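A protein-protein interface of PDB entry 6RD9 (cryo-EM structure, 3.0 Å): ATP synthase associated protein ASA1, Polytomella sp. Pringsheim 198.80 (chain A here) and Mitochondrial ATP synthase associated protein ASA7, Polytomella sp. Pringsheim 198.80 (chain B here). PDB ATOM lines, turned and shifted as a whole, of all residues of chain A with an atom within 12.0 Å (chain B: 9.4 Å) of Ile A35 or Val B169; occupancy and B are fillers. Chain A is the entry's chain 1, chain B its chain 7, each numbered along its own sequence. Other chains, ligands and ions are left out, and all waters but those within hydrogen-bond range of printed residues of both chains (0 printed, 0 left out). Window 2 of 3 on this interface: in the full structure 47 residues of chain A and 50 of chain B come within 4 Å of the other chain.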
ATOM      1  N   ASP A  30     -18.574 -24.584 -15.118  1.00  0.00           N
ATOM      2  CA  ASP A  30     -19.115 -24.302 -13.804  1.00  0.00           C
ATOM      3  C   ASP A  30     -18.044 -24.605 -12.778  1.00  0.00           C
ATOM      4  O   ASP A  30     -17.122 -25.381 -13.031  1.00  0.00           O
ATOM      5  CB  ASP A  30     -20.369 -25.114 -13.502  1.00  0.00           C
ATOM      6  CG  ASP A  30     -20.092 -26.586 -13.387  1.00  0.00           C
ATOM      7  OD1 ASP A  30     -19.647 -27.173 -14.382  1.00  0.00           O
ATOM      8  OD2 ASP A  30     -20.297 -27.160 -12.301  1.00  0.00           O
ATOM      9  N   PHE A  31     -18.182 -23.994 -11.617  1.00  0.00           N
ATOM     10  CA  PHE A  31     -17.144 -23.997 -10.609  1.00  0.00           C
ATOM     11  C   PHE A  31     -17.581 -24.822  -9.411  1.00  0.00           C
ATOM     12  O   PHE A  31     -18.765 -25.078  -9.203  1.00  0.00           O
ATOM     13  CB  PHE A  31     -16.818 -22.568 -10.189  1.00  0.00           C
ATOM     14  CG  PHE A  31     -16.121 -21.769 -11.243  1.00  0.00           C
ATOM     15  CD1 PHE A  31     -14.759 -21.608 -11.206  1.00  0.00           C
ATOM     16  CD2 PHE A  31     -16.826 -21.173 -12.267  1.00  0.00           C
ATOM     17  CE1 PHE A  31     -14.122 -20.878 -12.165  1.00  0.00           C
ATOM     18  CE2 PHE A  31     -16.184 -20.451 -13.230  1.00  0.00           C
ATOM     19  CZ  PHE A  31     -14.837 -20.304 -13.177  1.00  0.00           C
ATOM     20  N   THR A  32     -16.609 -25.255  -8.633  1.00  0.00           N
ATOM     21  CA  THR A  32     -16.861 -26.002  -7.412  1.00  0.00           C
ATOM     22  C   THR A  32     -16.665 -25.056  -6.241  1.00  0.00           C
ATOM     23  O   THR A  32     -15.540 -24.666  -5.935  1.00  0.00           O
ATOM     24  CB  THR A  32     -15.936 -27.208  -7.309  1.00  0.00           C
ATOM     25  OG1 THR A  32     -16.206 -28.093  -8.395  1.00  0.00           O
ATOM     26  CG2 THR A  32     -16.173 -27.949  -6.034  1.00  0.00           C
ATOM     27  N   GLU A  33     -17.758 -24.676  -5.595  1.00  0.00           N
ATOM     28  CA  GLU A  33     -17.661 -23.763  -4.471  1.00  0.00           C
ATOM     29  C   GLU A  33     -17.409 -24.464  -3.152  1.00  0.00           C
ATOM     30  O   GLU A  33     -16.794 -23.880  -2.264  1.00  0.00           O
ATOM     31  CB  GLU A  33     -18.920 -22.914  -4.381  1.00  0.00           C
ATOM     32  CG  GLU A  33     -18.898 -21.740  -5.324  1.00  0.00           C
ATOM     33  CD  GLU A  33     -19.438 -22.080  -6.685  1.00  0.00           C
ATOM     34  OE1 GLU A  33     -19.879 -23.230  -6.874  1.00  0.00           O
ATOM     35  OE2 GLU A  33     -19.421 -21.198  -7.569  1.00  0.00           O
ATOM     36  N   GLU A  34     -17.843 -25.701  -3.005  1.00  0.00           N
ATOM     37  CA  GLU A  34     -17.567 -26.442  -1.793  1.00  0.00           C
ATOM     38  C   GLU A  34     -16.139 -26.966  -1.804  1.00  0.00           C
ATOM     39  O   GLU A  34     -15.420 -26.869  -2.792  1.00  0.00           O
ATOM     40  CB  GLU A  34     -18.551 -27.597  -1.646  1.00  0.00           C
ATOM     41  CG  GLU A  34     -18.474 -28.627  -2.767  1.00  0.00           C
ATOM     42  CD  GLU A  34     -19.367 -28.310  -3.952  1.00  0.00           C
ATOM     43  OE1 GLU A  34     -19.941 -27.200  -3.997  1.00  0.00           O
ATOM     44  OE2 GLU A  34     -19.488 -29.172  -4.844  1.00  0.00           O
ATOM     45  N   ILE A  35     -15.710 -27.487  -0.666  1.00  0.00           N
ATOM     46  CA  ILE A  35     -14.492 -28.268  -0.562  1.00  0.00           C
ATOM     47  C   ILE A  35     -14.912 -29.524   0.177  1.00  0.00           C
ATOM     48  O   ILE A  35     -14.999 -29.531   1.407  1.00  0.00           O
ATOM     49  CB  ILE A  35     -13.366 -27.539   0.168  1.00  0.00           C
ATOM     50  CG1 ILE A  35     -12.969 -26.284  -0.581  1.00  0.00           C
ATOM     51  CG2 ILE A  35     -12.154 -28.411   0.284  1.00  0.00           C
ATOM     52  CD1 ILE A  35     -11.920 -25.509   0.107  1.00  0.00           C
ATOM     53  N   THR A  36     -15.213 -30.578  -0.567  1.00  0.00           N
ATOM     54  CA  THR A  36     -15.754 -31.801  -0.012  1.00  0.00           C
ATOM     55  C   THR A  36     -14.814 -32.963  -0.268  1.00  0.00           C
ATOM     56  O   THR A  36     -13.788 -32.836  -0.932  1.00  0.00           O
ATOM     57  CB  THR A  36     -17.128 -32.108  -0.603  1.00  0.00           C
ATOM     58  OG1 THR A  36     -17.055 -32.026  -2.027  1.00  0.00           O
ATOM     59  CG2 THR A  36     -18.169 -31.157  -0.083  1.00  0.00           C
ATOM     60  N   ALA A  37     -15.169 -34.094   0.319  1.00  0.00           N
ATOM     61  CA  ALA A  37     -14.512 -35.342   0.010  1.00  0.00           C
ATOM     62  C   ALA A  37     -15.021 -35.848  -1.338  1.00  0.00           C
ATOM     63  O   ALA A  37     -16.155 -35.563  -1.721  1.00  0.00           O
ATOM     64  CB  ALA A  37     -14.789 -36.358   1.112  1.00  0.00           C
ATOM     65  N   PRO A  38     -14.203 -36.587  -2.084  1.00  0.00           N
ATOM     66  CA  PRO A  38     -14.538 -36.832  -3.488  1.00  0.00           C
ATOM     67  C   PRO A  38     -15.487 -37.981  -3.807  1.00  0.00           C
ATOM     68  O   PRO A  38     -15.526 -38.368  -4.978  1.00  0.00           O
ATOM     69  CB  PRO A  38     -13.168 -37.094  -4.115  1.00  0.00           C
ATOM     70  CG  PRO A  38     -12.189 -36.684  -3.133  1.00  0.00           C
ATOM     71  CD  PRO A  38     -12.794 -36.906  -1.830  1.00  0.00           C
ATOM     72  N   LYS A  39     -16.231 -38.526  -2.835  1.00  0.00           N
ATOM     73  CA  LYS A  39     -17.323 -39.493  -3.049  1.00  0.00           C
ATOM     74  C   LYS A  39     -16.846 -40.795  -3.707  1.00  0.00           C
ATOM     75  O   LYS A  39     -17.135 -41.074  -4.868  1.00  0.00           O
ATOM     76  CB  LYS A  39     -18.460 -38.886  -3.877  1.00  0.00           C
ATOM     77  CG  LYS A  39     -19.354 -37.948  -3.123  1.00  0.00           C
ATOM     78  CD  LYS A  39     -20.194 -38.677  -2.104  1.00  0.00           C
ATOM     79  CE  LYS A  39     -20.973 -37.701  -1.249  1.00  0.00           C
ATOM     80  NZ  LYS A  39     -20.074 -36.828  -0.446  1.00  0.00           N
ATOM     81  N   ALA B 163     -14.458 -30.567 -13.318  1.00  0.00           N
ATOM     82  CA  ALA B 163     -15.216 -29.536 -12.631  1.00  0.00           C
ATOM     83  C   ALA B 163     -14.833 -29.426 -11.171  1.00  0.00           C
ATOM     84  O   ALA B 163     -14.994 -28.365 -10.575  1.00  0.00           O
ATOM     85  CB  ALA B 163     -16.704 -29.813 -12.755  1.00  0.00           C
ATOM     86  N   ARG B 164     -14.337 -30.501 -10.572  1.00  0.00           N
ATOM     87  CA  ARG B 164     -13.818 -30.408  -9.218  1.00  0.00           C
ATOM     88  C   ARG B 164     -12.491 -29.690  -9.188  1.00  0.00           C
ATOM     89  O   ARG B 164     -12.086 -29.181  -8.143  1.00  0.00           O
ATOM     90  CB  ARG B 164     -13.663 -31.788  -8.617  1.00  0.00           C
ATOM     91  CG  ARG B 164     -14.957 -32.439  -8.303  1.00  0.00           C
ATOM     92  CD  ARG B 164     -14.717 -33.784  -7.707  1.00  0.00           C
ATOM     93  NE  ARG B 164     -13.646 -33.744  -6.732  1.00  0.00           N
ATOM     94  CZ  ARG B 164     -13.830 -33.469  -5.452  1.00  0.00           C
ATOM     95  NH1 ARG B 164     -12.802 -33.454  -4.628  1.00  0.00           N
ATOM     96  NH2 ARG B 164     -15.041 -33.209  -5.000  1.00  0.00           N
ATOM     97  N   ARG B 165     -11.787 -29.664 -10.309  1.00  0.00           N
ATOM     98  CA  ARG B 165     -10.543 -28.930 -10.392  1.00  0.00           C
ATOM     99  C   ARG B 165     -10.762 -27.471 -10.709  1.00  0.00           C
ATOM    100  O   ARG B 165      -9.853 -26.669 -10.514  1.00  0.00           O
ATOM    101  CB  ARG B 165      -9.644 -29.529 -11.453  1.00  0.00           C
ATOM    102  CG  ARG B 165      -9.071 -30.872 -11.159  1.00  0.00           C
ATOM    103  CD  ARG B 165      -8.387 -30.903  -9.866  1.00  0.00           C
ATOM    104  NE  ARG B 165      -9.195 -31.641  -8.929  1.00  0.00           N
ATOM    105  CZ  ARG B 165      -8.883 -31.809  -7.662  1.00  0.00           C
ATOM    106  NH1 ARG B 165      -9.684 -32.494  -6.876  1.00  0.00           N
ATOM    107  NH2 ARG B 165      -7.771 -31.290  -7.188  1.00  0.00           N
ATOM    108  N   ARG B 166     -11.942 -27.101 -11.179  1.00  0.00           N
ATOM    109  CA  ARG B 166     -12.300 -25.700 -11.351  1.00  0.00           C
ATOM    110  C   ARG B 166     -12.865 -25.134 -10.067  1.00  0.00           C
ATOM    111  O   ARG B 166     -13.938 -24.561 -10.034  1.00  0.00           O
ATOM    112  CB  ARG B 166     -13.291 -25.544 -12.487  1.00  0.00           C
ATOM    113  CG  ARG B 166     -12.647 -25.425 -13.822  1.00  0.00           C
ATOM    114  CD  ARG B 166     -13.641 -24.943 -14.829  1.00  0.00           C
ATOM    115  NE  ARG B 166     -14.889 -25.681 -14.752  1.00  0.00           N
ATOM    116  CZ  ARG B 166     -15.121 -26.820 -15.385  1.00  0.00           C
ATOM    117  NH1 ARG B 166     -16.288 -27.420 -15.262  1.00  0.00           N
ATOM    118  NH2 ARG B 166     -14.192 -27.360 -16.139  1.00  0.00           N
ATOM    119  N   SER B 167     -12.121 -25.301  -8.990  1.00  0.00           N
ATOM    120  CA  SER B 167     -12.547 -24.829  -7.698  1.00  0.00           C
ATOM    121  C   SER B 167     -12.279 -23.345  -7.613  1.00  0.00           C
ATOM    122  O   SER B 167     -11.354 -22.829  -8.233  1.00  0.00           O
ATOM    123  CB  SER B 167     -11.805 -25.578  -6.601  1.00  0.00           C
ATOM    124  OG  SER B 167     -12.262 -25.214  -5.323  1.00  0.00           O
ATOM    125  N   THR B 168     -13.113 -22.651  -6.861  1.00  0.00           N
ATOM    126  CA  THR B 168     -12.929 -21.227  -6.657  1.00  0.00           C
ATOM    127  C   THR B 168     -11.870 -20.921  -5.617  1.00  0.00           C
ATOM    128  O   THR B 168     -11.564 -19.750  -5.395  1.00  0.00           O
ATOM    129  CB  THR B 168     -14.241 -20.594  -6.236  1.00  0.00           C
ATOM    130  OG1 THR B 168     -14.663 -21.178  -5.002  1.00  0.00           O
ATOM    131  CG2 THR B 168     -15.286 -20.847  -7.275  1.00  0.00           C
ATOM    132  N   VAL B 169     -11.307 -21.938  -4.978  1.00  0.00           N
ATOM    133  CA  VAL B 169     -10.276 -21.751  -3.975  1.00  0.00           C
ATOM    134  C   VAL B 169      -8.917 -22.034  -4.592  1.00  0.00           C
ATOM    135  O   VAL B 169      -8.064 -21.149  -4.651  1.00  0.00           O
ATOM    136  CB  VAL B 169     -10.534 -22.647  -2.763  1.00  0.00           C
ATOM    137  CG1 VAL B 169      -9.452 -22.491  -1.773  1.00  0.00           C
ATOM    138  CG2 VAL B 169     -11.830 -22.285  -2.144  1.00  0.00           C
ATOM    139  N   HIS B 170      -8.712 -23.256  -5.069  1.00  0.00           N
ATOM    140  CA  HIS B 170      -7.455 -23.685  -5.664  1.00  0.00           C
ATOM    141  C   HIS B 170      -7.712 -24.978  -6.409  1.00  0.00           C
ATOM    142  O   HIS B 170      -8.609 -25.729  -6.023  1.00  0.00           O
ATOM    143  CB  HIS B 170      -6.377 -23.894  -4.595  1.00  0.00           C
ATOM    144  CG  HIS B 170      -4.986 -23.940  -5.137  1.00  0.00           C
ATOM    145  ND1 HIS B 170      -4.179 -22.834  -5.210  1.00  0.00           N
ATOM    146  CD2 HIS B 170      -4.254 -24.965  -5.618  1.00  0.00           C
ATOM    147  CE1 HIS B 170      -3.015 -23.177  -5.727  1.00  0.00           C
ATOM    148  NE2 HIS B 170      -3.036 -24.464  -5.985  1.00  0.00           N
ATOM    149  N   PRO B 171      -6.972 -25.260  -7.484  1.00  0.00           N
ATOM    150  CA  PRO B 171      -7.086 -26.575  -8.128  1.00  0.00           C
ATOM    151  C   PRO B 171      -6.692 -27.743  -7.251  1.00  0.00           C
ATOM    152  O   PRO B 171      -7.275 -28.818  -7.379  1.00  0.00           O
ATOM    153  CB  PRO B 171      -6.136 -26.447  -9.313  1.00  0.00           C
ATOM    154  CG  PRO B 171      -6.104 -25.048  -9.598  1.00  0.00           C
ATOM    155  CD  PRO B 171      -6.288 -24.300  -8.354  1.00  0.00           C
ATOM    156  N   ALA B 172      -5.727 -27.559  -6.357  1.00  0.00           N
ATOM    157  CA  ALA B 172      -5.167 -28.613  -5.535  1.00  0.00           C
ATOM    158  C   ALA B 172      -5.701 -28.611  -4.122  1.00  0.00           C
ATOM    159  O   ALA B 172      -5.089 -29.218  -3.243  1.00  0.00           O
ATOM    160  CB  ALA B 172      -3.651 -28.491  -5.494  1.00  0.00           C
ATOM    161  N   ILE B 173      -6.800 -27.953  -3.873  1.00  0.00           N
ATOM    162  CA  ILE B 173      -7.320 -27.877  -2.518  1.00  0.00           C
ATOM    163  C   ILE B 173      -7.997 -29.193  -2.170  1.00  0.00           C
ATOM    164  O   ILE B 173      -8.461 -29.933  -3.040  1.00  0.00           O
ATOM    165  CB  ILE B 173      -8.266 -26.667  -2.376  1.00  0.00           C
ATOM    166  CG1 ILE B 173      -8.394 -26.225  -0.922  1.00  0.00           C
ATOM    167  CG2 ILE B 173      -9.617 -26.933  -2.986  1.00  0.00           C
ATOM    168  CD1 ILE B 173      -7.112 -25.933  -0.258  1.00  0.00           C
ATOM    169  N   GLY B 174      -7.989 -29.531  -0.886  1.00  0.00           N
ATOM    170  CA  GLY B 174      -8.694 -30.694  -0.400  1.00  0.00           C
ATOM    171  C   GLY B 174      -9.160 -30.457   1.017  1.00  0.00           C
ATOM    172  O   GLY B 174      -8.995 -29.372   1.555  1.00  0.00           O
ATOM    173  N   SER B 175      -9.731 -31.494   1.617  1.00  0.00           N
ATOM    174  CA  SER B 175     -10.289 -31.316   2.949  1.00  0.00           C
ATOM    175  C   SER B 175      -9.216 -31.256   4.017  1.00  0.00           C
ATOM    176  O   SER B 175      -9.346 -30.476   4.957  1.00  0.00           O
ATOM    177  CB  SER B 175     -11.277 -32.423   3.275  1.00  0.00           C
ATOM    178  OG  SER B 175     -12.454 -32.278   2.513  1.00  0.00           O
ATOM    179  N   THR B 176      -8.161 -32.060   3.901  1.00  0.00           N
ATOM    180  CA  THR B 176      -7.155 -32.111   4.955  1.00  0.00           C
ATOM    181  C   THR B 176      -6.383 -30.808   5.055  1.00  0.00           C
ATOM    182  O   THR B 176      -6.026 -30.377   6.152  1.00  0.00           O
ATOM    183  CB  THR B 176      -6.202 -33.268   4.709  1.00  0.00           C
ATOM    184  OG1 THR B 176      -6.959 -34.434   4.388  1.00  0.00           O
ATOM    185  CG2 THR B 176      -5.362 -33.548   5.931  1.00  0.00           C
ATOM    186  N   VAL B 177      -6.134 -30.152   3.928  1.00  0.00           N
ATOM    187  CA  VAL B 177      -5.473 -28.856   3.972  1.00  0.00           C
ATOM    188  C   VAL B 177      -6.438 -27.791   4.459  1.00  0.00           C
ATOM    189  O   VAL B 177      -6.098 -26.980   5.320  1.00  0.00           O
ATOM    190  CB  VAL B 177      -4.887 -28.517   2.594  1.00  0.00           C
ATOM    191  CG1 VAL B 177      -4.448 -27.095   2.529  1.00  0.00           C
ATOM    192  CG2 VAL B 177      -3.725 -29.399   2.321  1.00  0.00           C
ATOM    193  N   ALA B 178      -7.667 -27.803   3.964  1.00  0.00           N
ATOM    194  CA  ALA B 178      -8.625 -26.780   4.348  1.00  0.00           C
ATOM    195  C   ALA B 178      -9.155 -26.960   5.760  1.00  0.00           C
ATOM    196  O   ALA B 178      -9.743 -26.025   6.303  1.00  0.00           O
ATOM    197  CB  ALA B 178      -9.790 -26.751   3.372  1.00  0.00           C
ATOM    198  N   ASP B 179      -8.983 -28.135   6.360  1.00  0.00           N
ATOM    199  CA  ASP B 179      -9.249 -28.278   7.784  1.00  0.00           C
ATOM    200  C   ASP B 179      -8.058 -27.828   8.597  1.00  0.00           C
ATOM    201  O   ASP B 179      -8.220 -27.253   9.673  1.00  0.00           O
ATOM    202  CB  ASP B 179      -9.581 -29.722   8.126  1.00  0.00           C
ATOM    203  CG  ASP B 179     -10.918 -30.146   7.589  1.00  0.00           C
ATOM    204  OD1 ASP B 179     -11.618 -29.300   7.001  1.00  0.00           O
ATOM    205  OD2 ASP B 179     -11.266 -31.333   7.737  1.00  0.00           O
ATOM    206  N   ALA B 181      -6.098 -25.468   7.759  1.00  0.00           N
ATOM    207  CA  ALA B 181      -6.087 -24.025   7.696  1.00  0.00           C
ATOM    208  C   ALA B 181      -7.320 -23.402   8.314  1.00  0.00           C
ATOM    209  O   ALA B 181      -7.446 -22.180   8.304  1.00  0.00           O
ATOM    210  CB  ALA B 181      -5.954 -23.566   6.258  1.00  0.00           C
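N of Val B169 sits close to OG of Ser B167 (3.4 Å).
Of the printed residues of chain B, Phe A31 touches Arg B166 (3.3 Å) and Thr B168 (3.7 Å).
Of the printed residues of chain B, Thr A32 touches Ala B163 (2.5 Å), Arg B164 (3.4 Å), Arg B166 (3.1 Å), Ser B167 (3.4 Å) and Thr B168 (3.3 Å).
Glu A34 touches none of the printed residues of chain B.
Ile A35 touches just these residues of chain B: Val B169 (3.9 Å), Ile B173 (3.7 Å), Gly B174 (3.5 Å) and Ser B175 (3.9 Å).
Thr A36 touches just these residues of chain B: Arg B164 and Ser B175.
Ser B167 touches one residue of chain A.
Printed residues of chain A within 4 Å of Thr B168: Phe A31, Thr A32 and Glu A33.
Val B169 touches just one residue of chain A: Ile A35 (3.9 Å).
His B170 touches none of the printed residues of chain A.
Ala B172 touches none of the printed residues of chain A.
Of chain A, only Ile A35 (3.7 Å) comes within 4 Å of Ile B173.
Gly B174 touches just one residue of chain A: Ile A35.
The nearest residue of chain B that does not touch Ile A35 is Ala B178 (4.1 Å).
The nearest residue of chain A that does not touch Val B169 is Thr A32 (5.1 Å).
Among the printed residues, pairs that only touch across the chains: Phe A31 with Arg B166 (3.3 Å), Phe A31 with Thr B168 (3.7 Å), Thr A32 with Arg B164 (3.4 Å), Glu A33 with Thr B168 (3.99 Å), Ile A35 with Val B169 (3.9 Å), Ile A35 with Ile B173 (3.7 Å), Ile A35 with Gly B174 (3.5 Å), Ile A35 with Ser B175 (3.9 Å), Thr A36 with Arg B164 (3.8 Å), Thr A36 with Ser B175 (3.7 Å), Ala A37 with Ser B175 (3.9 Å) and Pro A38 with Arg B164 (3.6 Å).
The backbone carbonyl oxygen (O) of Thr A32 lies within hydrogen-bond range of the backbone NH (N) of Thr B168.
The backbone carbonyl oxygen (O) of Thr A32 lies within hydrogen-bond range of the side-chain hydroxyl (OG) of Ser B167 (3.4 Å).
The backbone carbonyl oxygen of Ala B163 is in hydrogen-bond range of the side-chain hydroxyl of Thr A32.
The backbone NH (N) of Thr A32 lies within hydrogen-bond range of the backbone carbonyl oxygen (O) of Arg B166 (3.1 Å).
The side-chain carboxylate (OD1) of Asp A30 lies within salt-bridge range of the guanidinium group (NH1) of Arg B166.
Of the 18 printed residues of chain B, 9 touch a printed residue of chain A.
Hydrophobic or aromatic side chains of chain A within 4 Å of the printed part of chain B: Phe A31, Ile A35 and Pro A38.
Among the printed residues, 17 pairs touch across the chains.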
